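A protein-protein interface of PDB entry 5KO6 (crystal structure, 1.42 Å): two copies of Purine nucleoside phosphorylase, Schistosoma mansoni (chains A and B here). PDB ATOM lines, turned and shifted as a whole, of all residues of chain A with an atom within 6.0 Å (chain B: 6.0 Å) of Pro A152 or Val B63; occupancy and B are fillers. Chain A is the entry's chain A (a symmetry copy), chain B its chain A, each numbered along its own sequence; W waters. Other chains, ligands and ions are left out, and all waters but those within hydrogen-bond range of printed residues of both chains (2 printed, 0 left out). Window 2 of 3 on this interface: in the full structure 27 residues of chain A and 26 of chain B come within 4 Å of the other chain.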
ATOM      1  N   VAL A   6      -4.727  -7.678  23.000  1.00  0.00           N
ATOM      2  CA  VAL A   6      -3.801  -6.553  23.109  1.00  0.00           C
ATOM      3  C   VAL A   6      -2.443  -6.958  22.549  1.00  0.00           C
ATOM      4  O   VAL A   6      -2.002  -8.095  22.724  1.00  0.00           O
ATOM      5  CB  VAL A   6      -3.703  -6.096  24.575  1.00  0.00           C
ATOM      6  CG1 VAL A   6      -2.652  -4.990  24.750  1.00  0.00           C
ATOM      7  CG2 VAL A   6      -5.056  -5.612  25.047  1.00  0.00           C
ATOM      8  N   GLN A  96      -4.345  -2.492  18.003  1.00  0.00           N
ATOM      9  CA  GLN A  96      -3.711  -3.691  18.543  1.00  0.00           C
ATOM     10  C   GLN A  96      -3.481  -4.724  17.454  1.00  0.00           C
ATOM     11  O   GLN A  96      -2.475  -5.450  17.469  1.00  0.00           O
ATOM     12  CB  GLN A  96      -4.568  -4.283  19.661  1.00  0.00           C
ATOM     13  CG  GLN A  96      -4.880  -3.331  20.833  1.00  0.00           C
ATOM     14  CD  GLN A  96      -3.641  -2.720  21.475  1.00  0.00           C
ATOM     15  OE1 GLN A  96      -2.561  -3.319  21.500  1.00  0.00           O
ATOM     16  NE2 GLN A  96      -3.796  -1.511  22.006  1.00  0.00           N
ATOM     17  N   LEU A 149      -0.550   4.200  17.783  1.00  0.00           N
ATOM     18  CA  LEU A 149      -0.109   3.984  19.157  1.00  0.00           C
ATOM     19  C   LEU A 149      -1.099   4.476  20.205  1.00  0.00           C
ATOM     20  O   LEU A 149      -0.808   4.332  21.402  1.00  0.00           O
ATOM     21  CB  LEU A 149       1.281   4.605  19.402  1.00  0.00           C
ATOM     22  CG  LEU A 149       2.469   3.816  18.830  1.00  0.00           C
ATOM     23  CD1 LEU A 149       3.758   4.642  18.967  1.00  0.00           C
ATOM     24  CD2 LEU A 149       2.636   2.465  19.544  1.00  0.00           C
ATOM     25  N   VAL A 150      -2.252   5.035  19.808  1.00  0.00           N
ATOM     26  CA  VAL A 150      -3.237   5.416  20.819  1.00  0.00           C
ATOM     27  C   VAL A 150      -3.645   4.181  21.604  1.00  0.00           C
ATOM     28  O   VAL A 150      -3.968   3.136  21.024  1.00  0.00           O
ATOM     29  CB  VAL A 150      -4.444   6.102  20.161  1.00  0.00           C
ATOM     30  CG1 VAL A 150      -5.595   6.276  21.176  1.00  0.00           C
ATOM     31  CG2 VAL A 150      -4.047   7.454  19.614  1.00  0.00           C
ATOM     32  N   GLY A 151      -3.655   4.312  22.929  1.00  0.00           N
ATOM     33  CA  GLY A 151      -3.893   3.216  23.837  1.00  0.00           C
ATOM     34  C   GLY A 151      -2.779   3.179  24.858  1.00  0.00           C
ATOM     35  O   GLY A 151      -1.854   3.999  24.824  1.00  0.00           O
ATOM     36  N   PRO A 152      -2.849   2.238  25.791  1.00  0.00           N
ATOM     37  CA  PRO A 152      -1.765   2.103  26.771  1.00  0.00           C
ATOM     38  C   PRO A 152      -0.460   1.825  26.049  1.00  0.00           C
ATOM     39  O   PRO A 152      -0.438   1.148  25.015  1.00  0.00           O
ATOM     40  CB  PRO A 152      -2.195   0.902  27.618  1.00  0.00           C
ATOM     41  CG  PRO A 152      -3.241   0.196  26.849  1.00  0.00           C
ATOM     42  CD  PRO A 152      -3.873   1.188  25.893  1.00  0.00           C
ATOM     43  N   ASN A 153       0.632   2.363  26.588  1.00  0.00           N
ATOM     44  CA  ASN A 153       1.936   2.021  26.039  1.00  0.00           C
ATOM     45  C   ASN A 153       2.361   0.628  26.477  1.00  0.00           C
ATOM     46  O   ASN A 153       2.200   0.253  27.639  1.00  0.00           O
ATOM     47  CB  ASN A 153       3.014   3.010  26.460  1.00  0.00           C
ATOM     48  CG  ASN A 153       4.292   2.802  25.670  1.00  0.00           C
ATOM     49  OD1 ASN A 153       4.273   2.850  24.428  1.00  0.00           O
ATOM     50  ND2 ASN A 153       5.380   2.528  26.355  1.00  0.00           N
ATOM     51  N   GLN A 154       2.937  -0.126  25.539  1.00  0.00           N
ATOM     52  CA  GLN A 154       3.545  -1.420  25.850  1.00  0.00           C
ATOM     53  C   GLN A 154       5.037  -1.171  26.063  1.00  0.00           C
ATOM     54  O   GLN A 154       5.827  -1.134  25.115  1.00  0.00           O
ATOM     55  CB  GLN A 154       3.263  -2.418  24.733  1.00  0.00           C
ATOM     56  CG  GLN A 154       1.777  -2.614  24.459  1.00  0.00           C
ATOM     57  CD  GLN A 154       0.996  -3.026  25.701  1.00  0.00           C
ATOM     58  OE1 GLN A 154       1.515  -3.693  26.593  1.00  0.00           O
ATOM     59  NE2 GLN A 154      -0.277  -2.629  25.755  1.00  0.00           N
ATOM     60  N   ARG A 160       6.709   5.697  25.603  1.00  0.00           N
ATOM     61  CA  ARG A 160       5.374   6.276  25.483  1.00  0.00           C
ATOM     62  C   ARG A 160       5.297   7.281  24.331  1.00  0.00           C
ATOM     63  O   ARG A 160       4.286   7.341  23.613  1.00  0.00           O
ATOM     64  CB  ARG A 160       4.993   6.933  26.819  1.00  0.00           C
ATOM     65  CG  ARG A 160       3.724   7.819  26.782  1.00  0.00           C
ATOM     66  CD  ARG A 160       2.398   7.042  26.776  1.00  0.00           C
ATOM     67  NE  ARG A 160       2.098   6.417  25.486  1.00  0.00           N
ATOM     68  CZ  ARG A 160       0.954   5.796  25.205  1.00  0.00           C
ATOM     69  NH1 ARG A 160       0.767   5.218  24.023  1.00  0.00           N
ATOM     70  NH2 ARG A 160      -0.005   5.725  26.129  1.00  0.00           N
ATOM     71  N   LYS B  60     -11.435   4.798  35.141  1.00  0.00           N
ATOM     72  CA  LYS B  60     -10.397   3.874  35.571  1.00  0.00           C
ATOM     73  C   LYS B  60      -9.077   4.281  34.928  1.00  0.00           C
ATOM     74  O   LYS B  60      -9.005   4.480  33.713  1.00  0.00           O
ATOM     75  CB  LYS B  60     -10.767   2.464  35.127  1.00  0.00           C
ATOM     76  CG  LYS B  60      -9.824   1.389  35.625  1.00  0.00           C
ATOM     77  CD  LYS B  60     -10.393  -0.001  35.345  1.00  0.00           C
ATOM     78  CE  LYS B  60      -9.532  -1.097  35.950  1.00  0.00           C
ATOM     79  NZ  LYS B  60      -9.441  -0.999  37.434  1.00  0.00           N
ATOM     80  N   THR B  61      -8.027   4.416  35.740  1.00  0.00           N
ATOM     81  CA  THR B  61      -6.727   4.834  35.224  1.00  0.00           C
ATOM     82  C   THR B  61      -5.622   3.843  35.567  1.00  0.00           C
ATOM     83  O   THR B  61      -4.439   4.171  35.402  1.00  0.00           O
ATOM     84  CB  THR B  61      -6.361   6.244  35.707  1.00  0.00           C
ATOM     85  OG1 THR B  61      -6.101   6.213  37.123  1.00  0.00           O
ATOM     86  CG2 THR B  61      -7.492   7.226  35.414  1.00  0.00           C
ATOM     87  N   THR B  62      -5.974   2.639  36.019  1.00  0.00           N
ATOM     88  CA  THR B  62      -4.970   1.677  36.453  1.00  0.00           C
ATOM     89  C   THR B  62      -4.193   1.058  35.296  1.00  0.00           C
ATOM     90  O   THR B  62      -3.080   0.576  35.512  1.00  0.00           O
ATOM     91  CB  THR B  62      -5.619   0.582  37.298  1.00  0.00           C
ATOM     92  OG1 THR B  62      -6.568  -0.136  36.505  1.00  0.00           O
ATOM     93  CG2 THR B  62      -6.332   1.190  38.495  1.00  0.00           C
ATOM     94  N   VAL B  63      -4.734   1.038  34.080  1.00  0.00           N
ATOM     95  CA  VAL B  63      -3.938   0.498  32.983  1.00  0.00           C
ATOM     96  C   VAL B  63      -2.726   1.387  32.719  1.00  0.00           C
ATOM     97  O   VAL B  63      -1.586   0.908  32.653  1.00  0.00           O
ATOM     98  CB  VAL B  63      -4.795   0.252  31.729  1.00  0.00           C
ATOM     99  CG1 VAL B  63      -3.906  -0.165  30.571  1.00  0.00           C
ATOM    100  CG2 VAL B  63      -5.814  -0.849  32.005  1.00  0.00           C
ATOM    101  N   ALA B  64      -2.948   2.699  32.607  1.00  0.00           N
ATOM    102  CA  ALA B  64      -1.819   3.621  32.516  1.00  0.00           C
ATOM    103  C   ALA B  64      -1.011   3.645  33.805  1.00  0.00           C
ATOM    104  O   ALA B  64       0.217   3.795  33.768  1.00  0.00           O
ATOM    105  CB  ALA B  64      -2.317   5.029  32.194  1.00  0.00           C
ATOM    106  N   GLY B  65      -1.675   3.490  34.947  1.00  0.00           N
ATOM    107  CA  GLY B  65      -1.029   3.600  36.232  1.00  0.00           C
ATOM    108  C   GLY B  65      -0.651   5.042  36.547  1.00  0.00           C
ATOM    109  O   GLY B  65      -1.198   6.008  36.000  1.00  0.00           O
ATOM    110  N   TYR B  90      -4.434  10.292  24.110  1.00  0.00           N
ATOM    111  CA  TYR B  90      -3.573   9.271  23.496  1.00  0.00           C
ATOM    112  C   TYR B  90      -3.494   7.995  24.327  1.00  0.00           C
ATOM    113  O   TYR B  90      -3.018   6.984  23.818  1.00  0.00           O
ATOM    114  CB  TYR B  90      -2.157   9.787  23.180  1.00  0.00           C
ATOM    115  CG  TYR B  90      -1.418  10.338  24.378  1.00  0.00           C
ATOM    116  CD1 TYR B  90      -0.954   9.506  25.386  1.00  0.00           C
ATOM    117  CD2 TYR B  90      -1.164  11.698  24.480  1.00  0.00           C
ATOM    118  CE1 TYR B  90      -0.290  10.023  26.488  1.00  0.00           C
ATOM    119  CE2 TYR B  90      -0.505  12.222  25.581  1.00  0.00           C
ATOM    120  CZ  TYR B  90      -0.074  11.375  26.575  1.00  0.00           C
ATOM    121  OH  TYR B  90       0.581  11.899  27.673  1.00  0.00           O
ATOM    122  N   GLU B  91      -3.935   8.017  25.589  1.00  0.00           N
ATOM    123  CA  GLU B  91      -3.970   6.788  26.377  1.00  0.00           C
ATOM    124  C   GLU B  91      -5.139   5.907  26.008  1.00  0.00           C
ATOM    125  O   GLU B  91      -5.180   4.745  26.430  1.00  0.00           O
ATOM    126  CB  GLU B  91      -4.128   7.113  27.867  1.00  0.00           C
ATOM    127  CG  GLU B  91      -2.875   7.636  28.510  1.00  0.00           C
ATOM    128  CD  GLU B  91      -1.714   6.609  28.606  1.00  0.00           C
ATOM    129  OE1 GLU B  91      -1.916   5.367  28.662  1.00  0.00           O
ATOM    130  OE2 GLU B  91      -0.566   7.071  28.633  1.00  0.00           O
ATOM    131  N   GLY B  92      -6.088   6.420  25.236  1.00  0.00           N
ATOM    132  CA  GLY B  92      -7.274   5.673  24.880  1.00  0.00           C
ATOM    133  C   GLY B  92      -8.504   6.014  25.686  1.00  0.00           C
ATOM    134  O   GLY B  92      -9.553   5.395  25.462  1.00  0.00           O
HETATM  135  O   HOH W   1       0.330   3.665  29.077  1.00  0.00           O
HETATM  136  O   HOH W   2       0.327   1.086  30.400  1.00  0.00           O
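O of Tyr B90 lies within hydrogen-bond range of N of Gly A151.
NH2 of Arg A160 lies within salt-bridge range of OE2 of Glu B91 (2.9 Å).
The backbone carbonyl oxygen (O) of Glu B91 lies close to the backbone nitrogen (N) of Pro A152, at 3.5 Å.
NH1 of Arg A160 lies within hydrogen-bond range of O of Leu A149.
The guanidinium group of Arg A160 is in hydrogen-bond range of the backbone carbonyl oxygen of Gly A151 (2.8 Å).
CA of Val A150 touches O of Tyr B90, 3.4 Å away.
Glu B91 touches Gly A151.
N of Gly B92 touches N of Gly A151 (3.96 Å).
CB of Pro A152 touches CG1 of Val B63, 3.6 Å away.
Arg A160 touches Tyr B90.
Of the printed residues of chain B, Pro A152 touches Val B63 and Glu B91.
Of chain A, only Pro A152 comes within 4 Å of Val B63.
Of the printed residues of chain A, Tyr B90 touches Val A150 (3.4 Å), Gly A151 (2.9 Å) and Arg A160 (3.97 Å).
Of the printed residues of chain B, Val A150 touches Tyr B90 (3.4 Å).
Of the printed residues of chain B, Gly A151 touches Tyr B90, Glu B91 and Gly B92.
Of the printed residues of chain B, Arg A160 touches Tyr B90 (3.97 Å) and Glu B91 (2.9 Å).
Thr B62 touches none of the printed residues of chain A.
The nearest printed residue of chain A that does not touch Val B63 is Asn A153 (6.3 Å).
The nearest printed residue of chain A that does not touch Gly B92 is Val A150 (4.1 Å).
Of the 9 printed residues of chain A, 4 touch a printed residue of chain B.
Hydrophobic or aromatic side chains of chain A that line the printed part of chain B: Val A150 and Pro A152.
Among the printed residues, 8 pairs touch across the chains.
Among the printed residues, Asp or Glu carboxylates within 4 Å of a Lys or Arg side-chain nitrogen of the other chain: Arg A160 with Glu B91 (2.9 Å).
No position is printed for both chains.
Water W1 bridges N of Asn A153 (2.8 Å) and OE1 of Glu B91 (2.8 Å).
Water W2 lies within hydrogen-bond range of O of Val B63 (3.0 Å) and O of Asn A153 (3.4 Å).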
